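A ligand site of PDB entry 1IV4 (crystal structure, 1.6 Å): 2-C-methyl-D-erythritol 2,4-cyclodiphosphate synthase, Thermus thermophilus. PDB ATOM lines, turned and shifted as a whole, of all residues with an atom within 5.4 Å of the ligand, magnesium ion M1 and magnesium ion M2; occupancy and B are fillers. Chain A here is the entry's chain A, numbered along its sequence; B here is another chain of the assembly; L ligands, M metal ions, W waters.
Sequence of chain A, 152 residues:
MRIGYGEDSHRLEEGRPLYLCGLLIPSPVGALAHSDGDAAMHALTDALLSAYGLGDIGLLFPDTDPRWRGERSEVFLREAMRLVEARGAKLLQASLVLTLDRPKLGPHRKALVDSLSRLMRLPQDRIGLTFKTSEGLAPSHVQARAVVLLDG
Magnesium ion M2 is bound by water W4.
NE2 of His 10 of chain B is bound to magnesium ion M2 (1.9 Å).
ND1 of His 42 of chain B binds magnesium ion M2 (2.0 Å).
Magnesium ion M2 is bound by OD2 of Asp 8 of chain B (2.0 Å).
Slightly farther from magnesium ion M2 lies the side-chain carboxylate (OD1) of Asp 8 of chain B (2.8 Å).
Water W1 lies within hydrogen-bond range of the backbone carbonyl oxygen of Ser 9 of chain B (2.7 Å), the side-chain carboxylate of Glu 135 (2.9 Å) and a ring nitrogen (ND1) of His 10 of chain B (3.3 Å).
Water W5 bridges an oxygen (O1) of the ligand (2.6 Å) and the backbone carbonyl oxygen of Ser 9 of chain B (3.4 Å).
Water W2 lies within hydrogen-bond range of NH2 of Arg 109 (2.8 Å) and O7 of the ligand (3.3 Å).
The backbone carbonyl oxygen (O) of Lys 132 sits at hydrogen-bond distance from the backbone NH (N) of Leu 100 (2.9 Å).
The side-chain hydroxyl (OG1) of Thr 133 is in hydrogen-bond range of the backbone NH (N) of Glu 135, 3.2 Å away.
OD1 of Asp 56 of chain B lies within hydrogen-bond range of N of Gly 58 of chain B.
The side-chain carboxylate (OD2) of Asp 56 of chain B is in hydrogen-bond range of the backbone NH (N) of Phe 131 (3.0 Å).
OD2 of Asp 56 of chain B lies within salt-bridge range of NH2 of Arg 109 (3.0 Å).
N of Leu 59 of chain B lies within hydrogen-bond range of OD1 of Asp 56 of chain B (3.1 Å).
The side-chain carboxylate of Asp 46 of chain B sits at hydrogen-bond distance from the backbone NH of Ile 57 of chain B, 2.7 Å away.
Water W4 is bound to magnesium ion M1, at 1.8 Å.
Water W1 binds magnesium ion M1 (2.0 Å).
NZ of Lys 132 binds magnesium ion M1.
O3 of the ligand binds magnesium ion M1 (2.1 Å).
The side-chain carboxylate (OD1) of Asp 8 of chain B binds magnesium ion M1, at 2.2 Å.
Water W5 is bound to magnesium ion M1 (2.2 Å).
Two residues have an atom within 4 Å of magnesium ion M1: Lys 132 and Asp 8 of chain B.
The backbone NH (N) of Thr 133 sits at hydrogen-bond distance from an oxygen (O1) of the ligand, 2.7 Å away.
O1 of the ligand is in hydrogen-bond range of OG1 of Thr 133.
An oxygen (O7) of the ligand lies within hydrogen-bond range of the side-chain carboxylate (OD1) of Asp 56 of chain B.
N of Leu 105 is in hydrogen-bond range of N2 of the ligand (2.8 Å).
The backbone NH (N) of Gly 106 is in hydrogen-bond range of an oxygen (O8) of the ligand (2.9 Å).
N of Gly 58 of chain B is in hydrogen-bond range of O6 of the ligand (2.9 Å).
N3 of the ligand is in hydrogen-bond range of O of Pro 103 (3.0 Å).
O of Leu 100 sits at hydrogen-bond distance from N3 of the ligand.
O7 of the ligand sits at hydrogen-bond distance from NH2 of Arg 109 (3.5 Å).
Within 4 Å of magnesium ion M2: Asp 8 of chain B, His 10 of chain B and His 42 of chain B.
The nearest printed residue that does not touch magnesium ion M2 is Lys 132 (4.3 Å).
The side-chain carboxylate (OE1) of Glu 135 sits close to an oxygen (O2) of the ligand, at 3.2 Å.
Residues that only touch the ligand: Lys 104, Phe 131, Ile 57 of chain B and Leu 59 of chain B.
Hydrophobic or aromatic side chains that line the ligand: Leu 100, Leu 105, Phe 131 and Ile 57 of chain B.
Of the 27 residues printed, 14 come within 4 Å of the ligand.
Along chain A the residues within 4 Å of the ligand span positions 100 to 135.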
ATOM      1  N   LEU A 100      -3.348   6.443 -13.155  1.00  0.00           N
ATOM      2  CA  LEU A 100      -3.945   5.886 -14.359  1.00  0.00           C
ATOM      3  C   LEU A 100      -2.927   4.964 -15.028  1.00  0.00           C
ATOM      4  O   LEU A 100      -1.717   5.192 -14.988  1.00  0.00           O
ATOM      5  CB  LEU A 100      -4.426   6.986 -15.300  1.00  0.00           C
ATOM      6  CG  LEU A 100      -3.332   7.716 -16.071  1.00  0.00           C
ATOM      7  CD1 LEU A 100      -3.941   8.587 -17.158  1.00  0.00           C
ATOM      8  CD2 LEU A 100      -2.482   8.515 -15.106  1.00  0.00           C
ATOM      9  N   ASP A 101      -3.454   3.900 -15.628  1.00  0.00           N
ATOM     10  CA  ASP A 101      -2.601   2.849 -16.144  1.00  0.00           C
ATOM     11  C   ASP A 101      -1.989   3.241 -17.475  1.00  0.00           C
ATOM     12  O   ASP A 101      -0.797   2.982 -17.661  1.00  0.00           O
ATOM     13  CB  ASP A 101      -3.372   1.537 -16.344  1.00  0.00           C
ATOM     14  CG  ASP A 101      -3.858   0.937 -15.046  1.00  0.00           C
ATOM     15  OD1 ASP A 101      -3.697   1.536 -13.972  1.00  0.00           O
ATOM     16  OD2 ASP A 101      -4.418  -0.176 -15.101  1.00  0.00           O
ATOM     17  N   ARG A 102      -2.812   3.819 -18.332  1.00  0.00           N
ATOM     18  CA  ARG A 102      -2.430   4.323 -19.651  1.00  0.00           C
ATOM     19  C   ARG A 102      -3.240   5.555 -19.984  1.00  0.00           C
ATOM     20  O   ARG A 102      -4.364   5.742 -19.450  1.00  0.00           O
ATOM     21  CB  ARG A 102      -2.637   3.222 -20.703  1.00  0.00           C
ATOM     22  CG  ARG A 102      -4.053   2.682 -20.663  1.00  0.00           C
ATOM     23  CD  ARG A 102      -4.295   1.446 -21.540  1.00  0.00           C
ATOM     24  NE  ARG A 102      -5.715   1.386 -21.899  1.00  0.00           N
ATOM     25  CZ  ARG A 102      -6.270   1.010 -23.028  1.00  0.00           C
ATOM     26  NH1 ARG A 102      -5.572   0.593 -24.082  1.00  0.00           N
ATOM     27  NH2 ARG A 102      -7.603   1.051 -23.107  1.00  0.00           N
ATOM     28  N   PRO A 103      -2.774   6.460 -20.829  1.00  0.00           N
ATOM     29  CA  PRO A 103      -1.448   6.399 -21.451  1.00  0.00           C
ATOM     30  C   PRO A 103      -0.323   6.782 -20.504  1.00  0.00           C
ATOM     31  O   PRO A 103      -0.573   7.298 -19.410  1.00  0.00           O
ATOM     32  CB  PRO A 103      -1.539   7.482 -22.540  1.00  0.00           C
ATOM     33  CG  PRO A 103      -2.471   8.493 -21.954  1.00  0.00           C
ATOM     34  CD  PRO A 103      -3.515   7.672 -21.251  1.00  0.00           C
ATOM     35  N   LYS A 104       0.926   6.539 -20.882  1.00  0.00           N
ATOM     36  CA  LYS A 104       2.050   7.068 -20.127  1.00  0.00           C
ATOM     37  C   LYS A 104       2.026   8.602 -20.159  1.00  0.00           C
ATOM     38  O   LYS A 104       1.885   9.186 -21.250  1.00  0.00           O
ATOM     39  CB  LYS A 104       3.387   6.574 -20.680  1.00  0.00           C
ATOM     40  CG  LYS A 104       3.344   5.244 -21.415  1.00  0.00           C
ATOM     41  CD  LYS A 104       3.185   4.059 -20.486  1.00  0.00           C
ATOM     42  CE  LYS A 104       4.273   4.009 -19.418  1.00  0.00           C
ATOM     43  NZ  LYS A 104       5.464   3.235 -19.886  1.00  0.00           N
ATOM     44  N   LEU A 105       2.174   9.233 -18.992  1.00  0.00           N
ATOM     45  CA  LEU A 105       2.115  10.689 -18.960  1.00  0.00           C
ATOM     46  C   LEU A 105       3.516  11.292 -18.962  1.00  0.00           C
ATOM     47  O   LEU A 105       3.659  12.474 -19.216  1.00  0.00           O
ATOM     48  CB  LEU A 105       1.346  11.224 -17.752  1.00  0.00           C
ATOM     49  CG  LEU A 105      -0.143  10.858 -17.705  1.00  0.00           C
ATOM     50  CD1 LEU A 105      -0.777  11.422 -16.442  1.00  0.00           C
ATOM     51  CD2 LEU A 105      -0.862  11.362 -18.943  1.00  0.00           C
ATOM     52  N   GLY A 106       4.528  10.471 -18.696  1.00  0.00           N
ATOM     53  CA  GLY A 106       5.904  10.980 -18.716  1.00  0.00           C
ATOM     54  C   GLY A 106       6.254  11.788 -19.944  1.00  0.00           C
ATOM     55  O   GLY A 106       6.856  12.874 -19.830  1.00  0.00           O
ATOM     56  N   PRO A 107       5.947  11.360 -21.170  1.00  0.00           N
ATOM     57  CA  PRO A 107       6.250  12.205 -22.335  1.00  0.00           C
ATOM     58  C   PRO A 107       5.584  13.570 -22.285  1.00  0.00           C
ATOM     59  O   PRO A 107       6.082  14.443 -23.017  1.00  0.00           O
ATOM     60  CB  PRO A 107       5.666  11.447 -23.538  1.00  0.00           C
ATOM     61  CG  PRO A 107       5.637  10.037 -23.065  1.00  0.00           C
ATOM     62  CD  PRO A 107       5.345  10.094 -21.586  1.00  0.00           C
ATOM     63  N   ARG A 109       5.076  15.305 -19.427  1.00  0.00           N
ATOM     64  CA  ARG A 109       5.333  15.951 -18.136  1.00  0.00           C
ATOM     65  C   ARG A 109       5.610  17.442 -18.231  1.00  0.00           C
ATOM     66  O   ARG A 109       5.040  18.211 -17.447  1.00  0.00           O
ATOM     67  CB  ARG A 109       6.507  15.231 -17.460  1.00  0.00           C
ATOM     68  CG  ARG A 109       6.678  15.566 -15.983  1.00  0.00           C
ATOM     69  CD  ARG A 109       7.908  14.869 -15.418  1.00  0.00           C
ATOM     70  NE  ARG A 109       7.789  13.420 -15.389  1.00  0.00           N
ATOM     71  CZ  ARG A 109       7.233  12.652 -14.452  1.00  0.00           C
ATOM     72  NH1 ARG A 109       6.712  13.242 -13.376  1.00  0.00           N
ATOM     73  NH2 ARG A 109       7.213  11.334 -14.579  1.00  0.00           N
ATOM     74  N   PHE A 131       3.021  10.949 -11.215  1.00  0.00           N
ATOM     75  CA  PHE A 131       2.121   9.999 -11.890  1.00  0.00           C
ATOM     76  C   PHE A 131       2.340   8.586 -11.373  1.00  0.00           C
ATOM     77  O   PHE A 131       3.471   8.174 -11.052  1.00  0.00           O
ATOM     78  CB  PHE A 131       2.392   9.950 -13.397  1.00  0.00           C
ATOM     79  CG  PHE A 131       2.602  11.285 -14.067  1.00  0.00           C
ATOM     80  CD1 PHE A 131       1.685  12.315 -13.929  1.00  0.00           C
ATOM     81  CD2 PHE A 131       3.729  11.531 -14.833  1.00  0.00           C
ATOM     82  CE1 PHE A 131       1.874  13.538 -14.542  1.00  0.00           C
ATOM     83  CE2 PHE A 131       3.916  12.738 -15.464  1.00  0.00           C
ATOM     84  CZ  PHE A 131       2.992  13.763 -15.333  1.00  0.00           C
ATOM     85  N   LYS A 132       1.261   7.800 -11.317  1.00  0.00           N
ATOM     86  CA  LYS A 132       1.431   6.387 -10.965  1.00  0.00           C
ATOM     87  C   LYS A 132       0.394   5.560 -11.723  1.00  0.00           C
ATOM     88  O   LYS A 132      -0.622   6.138 -12.105  1.00  0.00           O
ATOM     89  CB  LYS A 132       1.231   6.123  -9.495  1.00  0.00           C
ATOM     90  CG  LYS A 132       1.748   7.115  -8.484  1.00  0.00           C
ATOM     91  CD  LYS A 132       3.096   6.699  -7.927  1.00  0.00           C
ATOM     92  CE  LYS A 132       3.260   5.190  -7.814  1.00  0.00           C
ATOM     93  NZ  LYS A 132       4.699   4.784  -7.818  1.00  0.00           N
ATOM     94  N   THR A 133       0.626   4.269 -11.905  1.00  0.00           N
ATOM     95  CA  THR A 133      -0.426   3.374 -12.358  1.00  0.00           C
ATOM     96  C   THR A 133      -1.230   2.911 -11.151  1.00  0.00           C
ATOM     97  O   THR A 133      -0.825   3.151 -10.014  1.00  0.00           O
ATOM     98  CB  THR A 133       0.115   2.119 -13.085  1.00  0.00           C
ATOM     99  OG1 THR A 133       0.743   1.241 -12.121  1.00  0.00           O
ATOM    100  CG2 THR A 133       1.174   2.505 -14.095  1.00  0.00           C
ATOM    101  N   SER A 134      -2.344   2.237 -11.407  1.00  0.00           N
ATOM    102  CA  SER A 134      -3.148   1.665 -10.330  1.00  0.00           C
ATOM    103  C   SER A 134      -2.673   0.247  -9.992  1.00  0.00           C
ATOM    104  O   SER A 134      -3.212  -0.355  -9.077  1.00  0.00           O
ATOM    105  CB  SER A 134      -4.633   1.620 -10.711  1.00  0.00           C
ATOM    106  OG  SER A 134      -4.927   0.578 -11.621  1.00  0.00           O
ATOM    107  N   GLU A 135      -1.687  -0.252 -10.722  1.00  0.00           N
ATOM    108  CA  GLU A 135      -1.170  -1.597 -10.439  1.00  0.00           C
ATOM    109  C   GLU A 135      -2.321  -2.597 -10.541  1.00  0.00           C
ATOM    110  O   GLU A 135      -2.486  -3.561  -9.806  1.00  0.00           O
ATOM    111  CB  GLU A 135      -0.480  -1.707  -9.072  1.00  0.00           C
ATOM    112  CG  GLU A 135       0.827  -0.943  -8.975  1.00  0.00           C
ATOM    113  CD  GLU A 135       1.966  -1.424  -9.839  1.00  0.00           C
ATOM    114  OE1 GLU A 135       2.944  -0.660 -10.007  1.00  0.00           O
ATOM    115  OE2 GLU A 135       1.913  -2.556 -10.369  1.00  0.00           O
ATOM    116  N   ASP B   8       1.750   5.471  -3.416  1.00  0.00           N
ATOM    117  CA  ASP B   8       2.260   4.320  -4.167  1.00  0.00           C
ATOM    118  C   ASP B   8       1.374   3.136  -3.892  1.00  0.00           C
ATOM    119  O   ASP B   8       0.638   3.141  -2.904  1.00  0.00           O
ATOM    120  CB  ASP B   8       3.711   4.021  -3.776  1.00  0.00           C
ATOM    121  CG  ASP B   8       4.320   2.946  -4.658  1.00  0.00           C
ATOM    122  OD1 ASP B   8       3.971   2.908  -5.852  1.00  0.00           O
ATOM    123  OD2 ASP B   8       5.117   2.122  -4.159  1.00  0.00           O
ATOM    124  N   SER B   9       1.437   2.129  -4.755  1.00  0.00           N
ATOM    125  CA  SER B   9       0.730   0.895  -4.453  1.00  0.00           C
ATOM    126  C   SER B   9       1.427  -0.276  -5.156  1.00  0.00           C
ATOM    127  O   SER B   9       2.090  -0.025  -6.148  1.00  0.00           O
ATOM    128  CB  SER B   9      -0.738   0.880  -4.849  1.00  0.00           C
ATOM    129  OG  SER B   9      -0.911   1.247  -6.211  1.00  0.00           O
ATOM    130  N   HIS B  10       1.271  -1.458  -4.588  1.00  0.00           N
ATOM    131  CA  HIS B  10       1.834  -2.633  -5.248  1.00  0.00           C
ATOM    132  C   HIS B  10       0.923  -3.843  -5.037  1.00  0.00           C
ATOM    133  O   HIS B  10       0.329  -3.988  -3.986  1.00  0.00           O
ATOM    134  CB  HIS B  10       3.209  -3.011  -4.745  1.00  0.00           C
ATOM    135  CG  HIS B  10       4.262  -2.008  -5.086  1.00  0.00           C
ATOM    136  ND1 HIS B  10       4.967  -2.064  -6.273  1.00  0.00           N
ATOM    137  CD2 HIS B  10       4.715  -0.922  -4.423  1.00  0.00           C
ATOM    138  CE1 HIS B  10       5.825  -1.047  -6.309  1.00  0.00           C
ATOM    139  NE2 HIS B  10       5.697  -0.328  -5.203  1.00  0.00           N
ATOM    140  N   SER B  35      10.669  -3.700  -8.261  1.00  0.00           N
ATOM    141  CA  SER B  35      11.177  -3.029  -7.093  1.00  0.00           C
ATOM    142  C   SER B  35      11.133  -3.973  -5.889  1.00  0.00           C
ATOM    143  O   SER B  35      10.664  -5.105  -6.036  1.00  0.00           O
ATOM    144  CB  SER B  35      10.317  -1.787  -6.797  1.00  0.00           C
ATOM    145  OG  SER B  35       8.938  -2.051  -7.054  1.00  0.00           O
ATOM    146  N   GLY B  37       9.191  -3.060  -3.795  1.00  0.00           N
ATOM    147  CA  GLY B  37       7.775  -2.859  -3.562  1.00  0.00           C
ATOM    148  C   GLY B  37       7.410  -2.161  -2.267  1.00  0.00           C
ATOM    149  O   GLY B  37       6.271  -2.290  -1.834  1.00  0.00           O
ATOM    150  N   ASP B  38       8.357  -1.431  -1.693  1.00  0.00           N
ATOM    151  CA  ASP B  38       8.140  -0.741  -0.418  1.00  0.00           C
ATOM    152  C   ASP B  38       7.314   0.527  -0.645  1.00  0.00           C
ATOM    153  O   ASP B  38       7.853   1.595  -0.924  1.00  0.00           O
ATOM    154  CB  ASP B  38       9.456  -0.424   0.292  1.00  0.00           C
ATOM    155  CG  ASP B  38       9.341   0.056   1.718  1.00  0.00           C
ATOM    156  OD1 ASP B  38       8.374   0.764   2.060  1.00  0.00           O
ATOM    157  OD2 ASP B  38      10.270  -0.265   2.506  1.00  0.00           O
ATOM    158  N   ALA B  39       5.997   0.331  -0.516  1.00  0.00           N
ATOM    159  CA  ALA B  39       5.036   1.382  -0.819  1.00  0.00           C
ATOM    160  C   ALA B  39       5.251   2.624   0.022  1.00  0.00           C
ATOM    161  O   ALA B  39       5.076   3.757  -0.457  1.00  0.00           O
ATOM    162  CB  ALA B  39       3.613   0.857  -0.643  1.00  0.00           C
ATOM    163  N   HIS B  42       8.313   4.519  -1.244  1.00  0.00           N
ATOM    164  CA  HIS B  42       8.042   5.165  -2.532  1.00  0.00           C
ATOM    165  C   HIS B  42       7.142   6.381  -2.385  1.00  0.00           C
ATOM    166  O   HIS B  42       7.396   7.432  -3.000  1.00  0.00           O
ATOM    167  CB  HIS B  42       7.423   4.160  -3.509  1.00  0.00           C
ATOM    168  CG  HIS B  42       8.366   3.068  -3.901  1.00  0.00           C
ATOM    169  ND1 HIS B  42       7.991   2.020  -4.701  1.00  0.00           N
ATOM    170  CD2 HIS B  42       9.678   2.874  -3.610  1.00  0.00           C
ATOM    171  CE1 HIS B  42       9.028   1.196  -4.882  1.00  0.00           C
ATOM    172  NE2 HIS B  42      10.067   1.688  -4.231  1.00  0.00           N
ATOM    173  N   ASP B  46       8.237  10.145  -3.466  1.00  0.00           N
ATOM    174  CA  ASP B  46       7.455  10.968  -4.375  1.00  0.00           C
ATOM    175  C   ASP B  46       6.977  12.246  -3.668  1.00  0.00           C
ATOM    176  O   ASP B  46       6.970  13.318  -4.298  1.00  0.00           O
ATOM    177  CB  ASP B  46       6.234  10.229  -4.925  1.00  0.00           C
ATOM    178  CG  ASP B  46       6.530   9.523  -6.244  1.00  0.00           C
ATOM    179  OD1 ASP B  46       7.611   9.774  -6.823  1.00  0.00           O
ATOM    180  OD2 ASP B  46       5.676   8.740  -6.704  1.00  0.00           O
ATOM    181  N   ASP B  56       9.026  12.480 -10.276  1.00  0.00           N
ATOM    182  CA  ASP B  56       8.551  11.357  -9.473  1.00  0.00           C
ATOM    183  C   ASP B  56       9.579  10.232  -9.534  1.00  0.00           C
ATOM    184  O   ASP B  56      10.598  10.365 -10.241  1.00  0.00           O
ATOM    185  CB  ASP B  56       7.153  10.907  -9.889  1.00  0.00           C
ATOM    186  CG  ASP B  56       6.992  10.441 -11.314  1.00  0.00           C
ATOM    187  OD1 ASP B  56       7.902   9.729 -11.828  1.00  0.00           O
ATOM    188  OD2 ASP B  56       5.952  10.751 -11.965  1.00  0.00           O
ATOM    189  N   ILE B  57       9.365   9.170  -8.782  1.00  0.00           N
ATOM    190  CA  ILE B  57      10.371   8.093  -8.696  1.00  0.00           C
ATOM    191  C   ILE B  57      10.628   7.417 -10.037  1.00  0.00           C
ATOM    192  O   ILE B  57      11.744   6.908 -10.265  1.00  0.00           O
ATOM    193  CB  ILE B  57       9.964   7.042  -7.652  1.00  0.00           C
ATOM    194  CG1 ILE B  57       8.650   6.321  -7.930  1.00  0.00           C
ATOM    195  CG2 ILE B  57       9.970   7.667  -6.257  1.00  0.00           C
ATOM    196  CD1 ILE B  57       8.340   5.256  -6.905  1.00  0.00           C
ATOM    197  N   GLY B  58       9.627   7.407 -10.915  1.00  0.00           N
ATOM    198  CA  GLY B  58       9.770   6.783 -12.215  1.00  0.00           C
ATOM    199  C   GLY B  58      10.710   7.586 -13.085  1.00  0.00           C
ATOM    200  O   GLY B  58      11.457   7.043 -13.873  1.00  0.00           O
ATOM    201  N   LEU B  59      10.626   8.910 -12.930  1.00  0.00           N
ATOM    202  CA  LEU B  59      11.495   9.773 -13.688  1.00  0.00           C
ATOM    203  C   LEU B  59      12.917   9.731 -13.160  1.00  0.00           C
ATOM    204  O   LEU B  59      13.818   9.625 -14.016  1.00  0.00           O
ATOM    205  CB  LEU B  59      10.945  11.204 -13.681  1.00  0.00           C
ATOM    206  CG  LEU B  59      11.926  12.234 -14.251  1.00  0.00           C
ATOM    207  CD1 LEU B  59      12.037  12.070 -15.751  1.00  0.00           C
ATOM    208  CD2 LEU B  59      11.466  13.642 -13.825  1.00  0.00           C
HETATM  209  O1  LIG L   1       2.643   2.791 -10.896  1.00  0.00           O
HETATM  210  P1  LIG L   1       4.157   2.544 -11.242  1.00  0.00           P
HETATM  211  O2  LIG L   1       4.366   1.372 -12.052  1.00  0.00           O
HETATM  212  O3  LIG L   1       5.135   2.661  -9.982  1.00  0.00           O
HETATM  213  O4  LIG L   1       4.689   3.835 -12.046  1.00  0.00           O
HETATM  214  C1  LIG L   1       6.007   3.911 -12.518  1.00  0.00           C
HETATM  215  C2  LIG L   1       6.181   5.201 -13.178  1.00  0.00           C
HETATM  216  O5  LIG L   1       5.564   5.505 -14.449  1.00  0.00           O
HETATM  217  C3  LIG L   1       6.021   6.496 -12.341  1.00  0.00           C
HETATM  218  O6  LIG L   1       6.801   6.795 -11.154  1.00  0.00           O
HETATM  219  C4  LIG L   1       5.701   7.574 -13.349  1.00  0.00           C
HETATM  220  O7  LIG L   1       7.006   7.955 -13.705  1.00  0.00           O
HETATM  221  C5  LIG L   1       5.556   6.907 -14.654  1.00  0.00           C
HETATM  222  N1  LIG L   1       4.071   6.887 -15.088  1.00  0.00           N
HETATM  223  C6  LIG L   1       3.686   7.601 -16.286  1.00  0.00           C
HETATM  224  N2  LIG L   1       2.410   7.641 -16.755  1.00  0.00           N
HETATM  225  C7  LIG L   1       1.369   6.947 -16.085  1.00  0.00           C
HETATM  226  C8  LIG L   1       1.656   6.211 -14.878  1.00  0.00           C
HETATM  227  C9  LIG L   1       2.980   6.206 -14.452  1.00  0.00           C
HETATM  228  O8  LIG L   1       4.563   8.223 -16.911  1.00  0.00           O
HETATM  229  N3  LIG L   1       0.111   6.967 -16.559  1.00  0.00           N
HETATM  230 MG    MG M   1       4.554   2.724  -7.938  1.00  0.00          MG
HETATM  231 MG    MG M   2       6.313   1.449  -5.628  1.00  0.00          MG
HETATM  232  O   HOH W   1       4.128   0.735  -7.709  1.00  0.00           O
HETATM  233  O   HOH W   2       8.261   9.382 -16.349  1.00  0.00           O
HETATM  234  O   HOH W   3       8.085   0.463  -8.016  1.00  0.00           O
HETATM  235  O   HOH W   4       6.184   2.237  -7.332  1.00  0.00           O
HETATM  236  O   HOH W   5       2.369   2.595  -8.310  1.00  0.00           O
